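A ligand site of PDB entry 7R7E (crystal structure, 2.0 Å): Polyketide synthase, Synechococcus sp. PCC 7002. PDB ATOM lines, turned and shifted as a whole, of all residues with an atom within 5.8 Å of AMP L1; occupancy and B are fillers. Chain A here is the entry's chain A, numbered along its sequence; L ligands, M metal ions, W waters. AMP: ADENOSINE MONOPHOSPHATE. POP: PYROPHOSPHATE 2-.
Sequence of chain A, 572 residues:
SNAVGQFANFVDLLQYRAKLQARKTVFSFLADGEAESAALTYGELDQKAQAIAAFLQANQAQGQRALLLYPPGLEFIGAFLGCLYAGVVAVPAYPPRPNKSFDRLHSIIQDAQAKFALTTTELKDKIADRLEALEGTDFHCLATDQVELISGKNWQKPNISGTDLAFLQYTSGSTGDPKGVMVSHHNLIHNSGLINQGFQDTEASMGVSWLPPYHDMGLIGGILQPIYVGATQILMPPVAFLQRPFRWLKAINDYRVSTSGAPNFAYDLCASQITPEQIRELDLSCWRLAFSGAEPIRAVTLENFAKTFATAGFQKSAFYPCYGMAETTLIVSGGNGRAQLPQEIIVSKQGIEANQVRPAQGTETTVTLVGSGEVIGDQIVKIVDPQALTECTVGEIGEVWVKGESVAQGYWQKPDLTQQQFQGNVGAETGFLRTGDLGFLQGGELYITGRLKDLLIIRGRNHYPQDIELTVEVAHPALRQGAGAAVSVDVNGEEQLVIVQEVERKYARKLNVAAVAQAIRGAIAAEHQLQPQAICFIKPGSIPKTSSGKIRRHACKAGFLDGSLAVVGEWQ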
ATOM      1  N   THR A 171     -20.913  -0.203  28.127  1.00  0.00           N
ATOM      2  CA  THR A 171     -21.229   0.486  26.888  1.00  0.00           C
ATOM      3  C   THR A 171     -21.505  -0.551  25.813  1.00  0.00           C
ATOM      4  O   THR A 171     -21.242  -1.749  26.004  1.00  0.00           O
ATOM      5  CB  THR A 171     -20.062   1.384  26.425  1.00  0.00           C
ATOM      6  OG1 THR A 171     -18.940   0.572  26.030  1.00  0.00           O
ATOM      7  CG2 THR A 171     -19.605   2.320  27.539  1.00  0.00           C
ATOM      8  N   SER A 172     -22.056  -0.093  24.685  1.00  0.00           N
ATOM      9  CA  SER A 172     -22.602  -1.030  23.712  1.00  0.00           C
ATOM     10  C   SER A 172     -21.515  -1.786  22.972  1.00  0.00           C
ATOM     11  O   SER A 172     -21.744  -2.898  22.495  1.00  0.00           O
ATOM     12  CB  SER A 172     -23.519  -0.305  22.697  1.00  0.00           C
ATOM     13  OG  SER A 172     -24.701   0.165  23.334  1.00  0.00           O
ATOM     14  N   ASP A 216     -28.782   1.709  29.744  1.00  0.00           N
ATOM     15  CA  ASP A 216     -29.285   2.986  30.310  1.00  0.00           C
ATOM     16  C   ASP A 216     -30.725   3.374  29.970  1.00  0.00           C
ATOM     17  O   ASP A 216     -31.489   3.578  30.924  1.00  0.00           O
ATOM     18  CB  ASP A 216     -28.314   4.141  30.025  1.00  0.00           C
ATOM     19  CG  ASP A 216     -27.706   4.107  28.629  1.00  0.00           C
ATOM     20  OD1 ASP A 216     -28.417   3.706  27.684  1.00  0.00           O
ATOM     21  OD2 ASP A 216     -26.530   4.487  28.499  1.00  0.00           O
ATOM     22  N   SER A 292     -37.043  11.014  22.302  1.00  0.00           N
ATOM     23  CA  SER A 292     -36.213  10.358  21.262  1.00  0.00           C
ATOM     24  C   SER A 292     -34.746  10.626  21.576  1.00  0.00           C
ATOM     25  O   SER A 292     -34.396  11.796  21.726  1.00  0.00           O
ATOM     26  CB  SER A 292     -36.544  10.790  19.867  1.00  0.00           C
ATOM     27  OG  SER A 292     -35.832  10.008  18.918  1.00  0.00           O
ATOM     28  N   GLY A 293     -33.945   9.578  21.649  1.00  0.00           N
ATOM     29  CA  GLY A 293     -32.510   9.723  21.948  1.00  0.00           C
ATOM     30  C   GLY A 293     -31.787   8.432  21.687  1.00  0.00           C
ATOM     31  O   GLY A 293     -32.453   7.513  21.211  1.00  0.00           O
ATOM     32  N   ALA A 294     -30.477   8.376  21.970  1.00  0.00           N
ATOM     33  CA  ALA A 294     -29.630   7.177  21.761  1.00  0.00           C
ATOM     34  C   ALA A 294     -29.114   7.124  20.324  1.00  0.00           C
ATOM     35  O   ALA A 294     -28.268   6.274  20.036  1.00  0.00           O
ATOM     36  CB  ALA A 294     -30.297   5.905  22.175  1.00  0.00           C
ATOM     37  N   GLU A 295     -29.562   8.050  19.492  1.00  0.00           N
ATOM     38  CA  GLU A 295     -29.149   8.048  18.073  1.00  0.00           C
ATOM     39  C   GLU A 295     -29.460   9.406  17.425  1.00  0.00           C
ATOM     40  O   GLU A 295     -30.244  10.154  18.017  1.00  0.00           O
ATOM     41  CB  GLU A 295     -29.733   6.856  17.315  1.00  0.00           C
ATOM     42  CG  GLU A 295     -31.131   7.048  16.776  1.00  0.00           C
ATOM     43  CD  GLU A 295     -31.493   6.012  15.719  1.00  0.00           C
ATOM     44  OE1 GLU A 295     -30.827   6.000  14.670  1.00  0.00           O
ATOM     45  OE2 GLU A 295     -32.418   5.230  15.950  1.00  0.00           O
ATOM     46  N   PRO A 296     -28.867   9.775  16.268  1.00  0.00           N
ATOM     47  CA  PRO A 296     -29.232  11.034  15.632  1.00  0.00           C
ATOM     48  C   PRO A 296     -30.740  11.216  15.454  1.00  0.00           C
ATOM     49  O   PRO A 296     -31.383  10.317  15.005  1.00  0.00           O
ATOM     50  CB  PRO A 296     -28.449  10.983  14.302  1.00  0.00           C
ATOM     51  CG  PRO A 296     -27.254  10.111  14.605  1.00  0.00           C
ATOM     52  CD  PRO A 296     -27.776   9.089  15.592  1.00  0.00           C
ATOM     53  N   ILE A 297     -31.269  12.363  15.862  1.00  0.00           N
ATOM     54  CA  ILE A 297     -32.687  12.708  15.698  1.00  0.00           C
ATOM     55  C   ILE A 297     -32.820  13.394  14.345  1.00  0.00           C
ATOM     56  O   ILE A 297     -32.295  14.497  14.137  1.00  0.00           O
ATOM     57  CB  ILE A 297     -33.196  13.588  16.839  1.00  0.00           C
ATOM     58  CG1 ILE A 297     -32.977  12.891  18.202  1.00  0.00           C
ATOM     59  CG2 ILE A 297     -34.655  13.963  16.646  1.00  0.00           C
ATOM     60  CD1 ILE A 297     -32.712  13.809  19.420  1.00  0.00           C
ATOM     61  N   CYS A 322     -33.629  14.282  23.324  1.00  0.00           N
ATOM     62  CA  CYS A 322     -32.737  14.277  24.478  1.00  0.00           C
ATOM     63  C   CYS A 322     -31.420  13.630  24.104  1.00  0.00           C
ATOM     64  O   CYS A 322     -31.295  12.942  23.083  1.00  0.00           O
ATOM     65  CB  CYS A 322     -33.408  13.575  25.700  1.00  0.00           C
ATOM     66  SG  CYS A 322     -34.050  11.947  25.345  1.00  0.00           S
ATOM     67  N   TYR A 323     -30.405  13.915  24.925  1.00  0.00           N
ATOM     68  CA  TYR A 323     -29.061  13.411  24.703  1.00  0.00           C
ATOM     69  C   TYR A 323     -28.487  12.962  26.032  1.00  0.00           C
ATOM     70  O   TYR A 323     -28.660  13.640  27.058  1.00  0.00           O
ATOM     71  CB  TYR A 323     -28.164  14.481  24.036  1.00  0.00           C
ATOM     72  CG  TYR A 323     -26.658  14.254  24.139  1.00  0.00           C
ATOM     73  CD1 TYR A 323     -26.020  13.311  23.346  1.00  0.00           C
ATOM     74  CD2 TYR A 323     -25.897  14.959  25.070  1.00  0.00           C
ATOM     75  CE1 TYR A 323     -24.645  13.088  23.429  1.00  0.00           C
ATOM     76  CE2 TYR A 323     -24.496  14.756  25.168  1.00  0.00           C
ATOM     77  CZ  TYR A 323     -23.889  13.814  24.354  1.00  0.00           C
ATOM     78  OH  TYR A 323     -22.517  13.600  24.423  1.00  0.00           O
ATOM     79  N   GLY A 324     -27.837  11.811  26.010  1.00  0.00           N
ATOM     80  CA  GLY A 324     -27.068  11.323  27.138  1.00  0.00           C
ATOM     81  C   GLY A 324     -26.313  10.067  26.749  1.00  0.00           C
ATOM     82  O   GLY A 324     -26.401   9.575  25.615  1.00  0.00           O
ATOM     83  N   MET A 325     -25.590   9.521  27.733  1.00  0.00           N
ATOM     84  CA  MET A 325     -24.749   8.355  27.526  1.00  0.00           C
ATOM     85  C   MET A 325     -24.533   7.615  28.850  1.00  0.00           C
ATOM     86  O   MET A 325     -24.771   8.154  29.933  1.00  0.00           O
ATOM     87  CB  MET A 325     -23.470   8.824  26.872  1.00  0.00           C
ATOM     88  CG  MET A 325     -22.614   9.562  27.825  1.00  0.00           C
ATOM     89  SD  MET A 325     -21.266  10.495  27.004  1.00  0.00           S
ATOM     90  CE  MET A 325     -20.425   9.252  25.916  1.00  0.00           C
ATOM     91  N   ALA A 326     -23.967   6.410  28.749  1.00  0.00           N
ATOM     92  CA  ALA A 326     -23.767   5.611  29.950  1.00  0.00           C
ATOM     93  C   ALA A 326     -22.842   6.324  30.916  1.00  0.00           C
ATOM     94  O   ALA A 326     -23.100   6.345  32.130  1.00  0.00           O
ATOM     95  CB  ALA A 326     -23.238   4.224  29.599  1.00  0.00           C
ATOM     96  N   GLU A 327     -21.785   6.979  30.387  1.00  0.00           N
ATOM     97  CA  GLU A 327     -20.800   7.710  31.207  1.00  0.00           C
ATOM     98  C   GLU A 327     -21.425   8.893  31.959  1.00  0.00           C
ATOM     99  O   GLU A 327     -20.845   9.388  32.941  1.00  0.00           O
ATOM    100  CB  GLU A 327     -19.614   8.243  30.342  1.00  0.00           C
ATOM    101  CG  GLU A 327     -18.633   7.164  29.858  1.00  0.00           C
ATOM    102  CD  GLU A 327     -19.059   6.561  28.510  1.00  0.00           C
ATOM    103  OE1 GLU A 327     -20.259   6.759  28.121  1.00  0.00           O
ATOM    104  OE2 GLU A 327     -18.167   5.955  27.826  1.00  0.00           O
ATOM    105  N   LEU A 330     -27.379   8.743  32.553  1.00  0.00           N
ATOM    106  CA  LEU A 330     -28.251   8.762  31.382  1.00  0.00           C
ATOM    107  C   LEU A 330     -28.302  10.186  30.792  1.00  0.00           C
ATOM    108  O   LEU A 330     -27.394  10.593  30.050  1.00  0.00           O
ATOM    109  CB  LEU A 330     -29.660   8.226  31.759  1.00  0.00           C
ATOM    110  CG  LEU A 330     -30.689   8.039  30.637  1.00  0.00           C
ATOM    111  CD1 LEU A 330     -30.107   7.249  29.516  1.00  0.00           C
ATOM    112  CD2 LEU A 330     -31.947   7.317  31.164  1.00  0.00           C
ATOM    113  N   SER A 372     -30.814  18.622  20.460  1.00  0.00           N
ATOM    114  CA  SER A 372     -31.070  17.553  21.420  1.00  0.00           C
ATOM    115  C   SER A 372     -31.442  18.072  22.807  1.00  0.00           C
ATOM    116  O   SER A 372     -31.230  17.360  23.784  1.00  0.00           O
ATOM    117  CB  SER A 372     -29.871  16.618  21.533  1.00  0.00           C
ATOM    118  OG  SER A 372     -29.906  15.680  20.485  1.00  0.00           O
ATOM    119  N   THR A 435     -16.904  13.257  26.188  1.00  0.00           N
ATOM    120  CA  THR A 435     -17.937  12.325  25.722  1.00  0.00           C
ATOM    121  C   THR A 435     -17.516  11.547  24.496  1.00  0.00           C
ATOM    122  O   THR A 435     -18.075  10.466  24.242  1.00  0.00           O
ATOM    123  CB  THR A 435     -19.244  13.053  25.394  1.00  0.00           C
ATOM    124  OG1 THR A 435     -19.044  13.986  24.305  1.00  0.00           O
ATOM    125  CG2 THR A 435     -19.810  13.743  26.635  1.00  0.00           C
ATOM    126  N   ASP A 437     -18.322  12.759  21.661  1.00  0.00           N
ATOM    127  CA  ASP A 437     -19.274  13.216  20.673  1.00  0.00           C
ATOM    128  C   ASP A 437     -18.893  14.611  20.193  1.00  0.00           C
ATOM    129  O   ASP A 437     -18.407  15.440  20.967  1.00  0.00           O
ATOM    130  CB  ASP A 437     -20.710  13.205  21.229  1.00  0.00           C
ATOM    131  CG  ASP A 437     -21.180  11.798  21.603  1.00  0.00           C
ATOM    132  OD1 ASP A 437     -21.108  10.901  20.724  1.00  0.00           O
ATOM    133  OD2 ASP A 437     -21.716  11.602  22.738  1.00  0.00           O
ATOM    134  N   ILE A 448     -25.886  17.677  18.459  1.00  0.00           N
ATOM    135  CA  ILE A 448     -24.873  16.627  18.330  1.00  0.00           C
ATOM    136  C   ILE A 448     -24.723  16.310  16.845  1.00  0.00           C
ATOM    137  O   ILE A 448     -25.712  15.983  16.186  1.00  0.00           O
ATOM    138  CB  ILE A 448     -25.296  15.362  19.099  1.00  0.00           C
ATOM    139  CG1 ILE A 448     -25.585  15.665  20.577  1.00  0.00           C
ATOM    140  CG2 ILE A 448     -24.224  14.312  18.918  1.00  0.00           C
ATOM    141  CD1 ILE A 448     -24.397  16.166  21.324  1.00  0.00           C
ATOM    142  N   GLY A 450     -22.050  14.014  15.690  1.00  0.00           N
ATOM    143  CA  GLY A 450     -21.643  12.630  15.531  1.00  0.00           C
ATOM    144  C   GLY A 450     -20.575  12.219  16.523  1.00  0.00           C
ATOM    145  O   GLY A 450     -20.284  12.949  17.474  1.00  0.00           O
ATOM    146  N   ARG A 451     -20.035  11.009  16.294  1.00  0.00           N
ATOM    147  CA  ARG A 451     -18.987  10.435  17.128  1.00  0.00           C
ATOM    148  C   ARG A 451     -17.632  10.806  16.563  1.00  0.00           C
ATOM    149  O   ARG A 451     -17.418  10.694  15.364  1.00  0.00           O
ATOM    150  CB  ARG A 451     -19.089   8.910  17.238  1.00  0.00           C
ATOM    151  CG  ARG A 451     -20.527   8.410  17.409  1.00  0.00           C
ATOM    152  CD  ARG A 451     -20.517   6.925  17.769  1.00  0.00           C
ATOM    153  NE  ARG A 451     -21.809   6.472  18.291  1.00  0.00           N
ATOM    154  CZ  ARG A 451     -21.974   5.815  19.432  1.00  0.00           C
ATOM    155  NH1 ARG A 451     -20.957   5.574  20.244  1.00  0.00           N
ATOM    156  NH2 ARG A 451     -23.195   5.383  19.753  1.00  0.00           N
ATOM    157  N   LYS A 550     -26.805  -1.720  17.177  1.00  0.00           N
ATOM    158  CA  LYS A 550     -25.997  -0.645  16.600  1.00  0.00           C
ATOM    159  C   LYS A 550     -24.861  -1.202  15.760  1.00  0.00           C
ATOM    160  O   LYS A 550     -24.172  -2.128  16.172  1.00  0.00           O
ATOM    161  CB  LYS A 550     -25.398   0.254  17.683  1.00  0.00           C
ATOM    162  CG  LYS A 550     -26.384   0.833  18.678  1.00  0.00           C
ATOM    163  CD  LYS A 550     -25.604   1.553  19.773  1.00  0.00           C
ATOM    164  CE  LYS A 550     -26.503   1.998  20.916  1.00  0.00           C
ATOM    165  NZ  LYS A 550     -25.757   2.482  22.120  1.00  0.00           N
HETATM  166  P   AMP L   1     -24.990   4.809  25.278  1.00  0.00           P
HETATM  167  O1P AMP L   1     -25.209   3.420  24.787  1.00  0.00           O
HETATM  168  O2P AMP L   1     -26.214   5.473  25.803  1.00  0.00           O
HETATM  169  O3P AMP L   1     -23.787   4.997  26.132  1.00  0.00           O
HETATM  170  O5' AMP L   1     -24.657   5.591  23.926  1.00  0.00           O
HETATM  171  C5' AMP L   1     -24.324   6.972  23.956  1.00  0.00           C
HETATM  172  C4' AMP L   1     -24.140   7.498  22.551  1.00  0.00           C
HETATM  173  O4' AMP L   1     -25.327   7.462  21.767  1.00  0.00           O
HETATM  174  C3' AMP L   1     -23.783   8.957  22.583  1.00  0.00           C
HETATM  175  O3' AMP L   1     -22.429   9.121  22.903  1.00  0.00           O
HETATM  176  C2' AMP L   1     -24.075   9.354  21.172  1.00  0.00           C
HETATM  177  O2' AMP L   1     -23.028   8.928  20.307  1.00  0.00           O
HETATM  178  C1' AMP L   1     -25.323   8.565  20.858  1.00  0.00           C
HETATM  179  N9  AMP L   1     -26.430   9.487  21.126  1.00  0.00           N
HETATM  180  C8  AMP L   1     -27.196   9.544  22.229  1.00  0.00           C
HETATM  181  N7  AMP L   1     -28.113  10.521  22.149  1.00  0.00           N
HETATM  182  C5  AMP L   1     -27.923  11.119  20.973  1.00  0.00           C
HETATM  183  C6  AMP L   1     -28.547  12.239  20.275  1.00  0.00           C
HETATM  184  N6  AMP L   1     -29.572  12.900  20.833  1.00  0.00           N
HETATM  185  N1  AMP L   1     -28.055  12.569  19.066  1.00  0.00           N
HETATM  186  C2  AMP L   1     -27.033  11.908  18.522  1.00  0.00           C
HETATM  187  N3  AMP L   1     -26.414  10.872  19.101  1.00  0.00           N
HETATM  188  C4  AMP L   1     -26.817  10.445  20.308  1.00  0.00           C
HETATM  189  P1  POP L   2     -19.304   2.357  22.937  1.00  0.00           P
HETATM  190  O1  POP L   2     -18.821   1.044  23.406  1.00  0.00           O
HETATM  191  O2  POP L   2     -19.133   3.394  24.005  1.00  0.00           O
HETATM  192  O3  POP L   2     -18.464   2.666  21.756  1.00  0.00           O
HETATM  193  O   POP L   2     -20.815   2.310  22.404  1.00  0.00           O
HETATM  194  P2  POP L   2     -21.990   3.273  22.856  1.00  0.00           P
HETATM  195  O4  POP L   2     -22.475   2.761  24.178  1.00  0.00           O
HETATM  196  O5  POP L   2     -21.560   4.695  22.988  1.00  0.00           O
HETATM  197  O6  POP L   2     -23.046   3.197  21.807  1.00  0.00           O
HETATM  198 MG    MG M   1     -19.859   5.325  24.023  1.00  0.00          MG
HETATM  199  O   HOH W   1     -21.153   5.392  25.878  1.00  0.00           O
HETATM  200  O   HOH W   2     -23.935  10.031  17.763  1.00  0.00           O
HETATM  201  O   HOH W   3     -29.094  14.177  17.039  1.00  0.00           O
HETATM  202  O   HOH W   4     -20.720   7.296  23.465  1.00  0.00           O
HETATM  203  O   HOH W   5     -26.530   4.955  22.103  1.00  0.00           O
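A nitrogen (N1) of AMP L1 sits close to the backbone carbonyl oxygen of Glu 295, at 3.4 Å. Ser 172 touches AMP L1 (OG to O1P, 3.6 Å). N of Pro 296 touches C2 of AMP L1, 3.6 Å away. CD1 of Ile 297 touches N6 of AMP L1, 3.6 Å away. Tyr 323 touches AMP L1. O of Gly 324 touches C8 of AMP L1, at 3.5 Å. CB of Met 325 touches C5' of AMP L1, at 3.6 Å. Ile 448 touches AMP L1 (CG2 to C2, 3.7 Å). Hydrophobic or aromatic side chains within 4 Å of AMP L1: Ile 297, Tyr 323, Met 325, Ala 326 and Ile 448. 16 residues have an atom within 4 Å of AMP L1: Ser 172, Asp 216, Ala 294, Glu 295, Pro 296, Ile 297, Cys 322, Tyr 323, Gly 324, Met 325, Ala 326, Ser 372, Asp 437, Ile 448, Arg 451 and Lys 550.
The side-chain carboxylate (OD2) of Asp 437 is in hydrogen-bond range of the side-chain hydroxyl (OH) of Tyr 323 (2.7 Å). The backbone NH (N) of Asp 437 sits at hydrogen-bond distance from the side-chain hydroxyl (OG1) of Thr 435 (3.0 Å). The backbone NH (N) of Cys 322 sits at hydrogen-bond distance from the backbone carbonyl oxygen (O) of Ser 292 (3.1 Å). The side-chain amino group of Lys 550 is in hydrogen-bond range of the side-chain hydroxyl of Ser 172. The side-chain carboxylate (OD2) of Asp 216 lies within hydrogen-bond range of the backbone NH (N) of Ala 326 (3.2 Å). The backbone NH of Met 325 lies within hydrogen-bond range of the backbone carbonyl oxygen of Leu 330, at 3.1 Å. OH of Tyr 323 lies close to OG1 of Thr 435 (3.5 Å).
The side-chain carboxylate (OD2) of Asp 437 sits at hydrogen-bond distance from an oxygen (O3') of AMP L1 (2.6 Å). The side-chain hydroxyl (OG) of Ser 372 is in hydrogen-bond range of a nitrogen (N6) of AMP L1, at 2.8 Å. N6 of AMP L1 lies within hydrogen-bond range of O of Cys 322 (2.8 Å). The side-chain amino group of Lys 550 is in salt-bridge range of an oxygen (O1P) of AMP L1 (2.9 Å). OD2 of Asp 216 lies close to O2P of AMP L1 (2.9 Å). The backbone NH (N) of Ala 326 is in hydrogen-bond range of an oxygen (O3P) of AMP L1 (3.0 Å). The backbone NH of Ala 294 sits at hydrogen-bond distance from a nitrogen (N7) of AMP L1, 3.2 Å away. NE of Arg 451 lies close to O2' of AMP L1 (3.4 Å). The side-chain amino group (NZ) of Lys 550 is in salt-bridge range of an oxygen (O6) of POP L2, 2.8 Å away. O6 of POP L2 is in salt-bridge range of NH2 of Arg 451 (3.0 Å). N of Ser 172 lies within hydrogen-bond range of O4 of POP L2. O1 of POP L2 lies within hydrogen-bond range of OG1 of Thr 171 (2.7 Å).
O1P of AMP L1 lies close to O4 of POP L2 (2.9 Å).
Water W1 lies within hydrogen-bond range of O3P of AMP L1 (2.7 Å), OE1 of Glu 327 (2.8 Å) and O4 of POP L2 (3.4 Å). Water W5 lies within hydrogen-bond range of the side-chain amino group (NZ) of Lys 550 (2.6 Å), an oxygen (O5') of AMP L1 (2.7 Å) and the backbone carbonyl oxygen (O) of Ala 294 (3.0 Å). Water W3 lies within hydrogen-bond range of N1 of AMP L1 (2.8 Å) and N of Ile 297 (3.1 Å).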
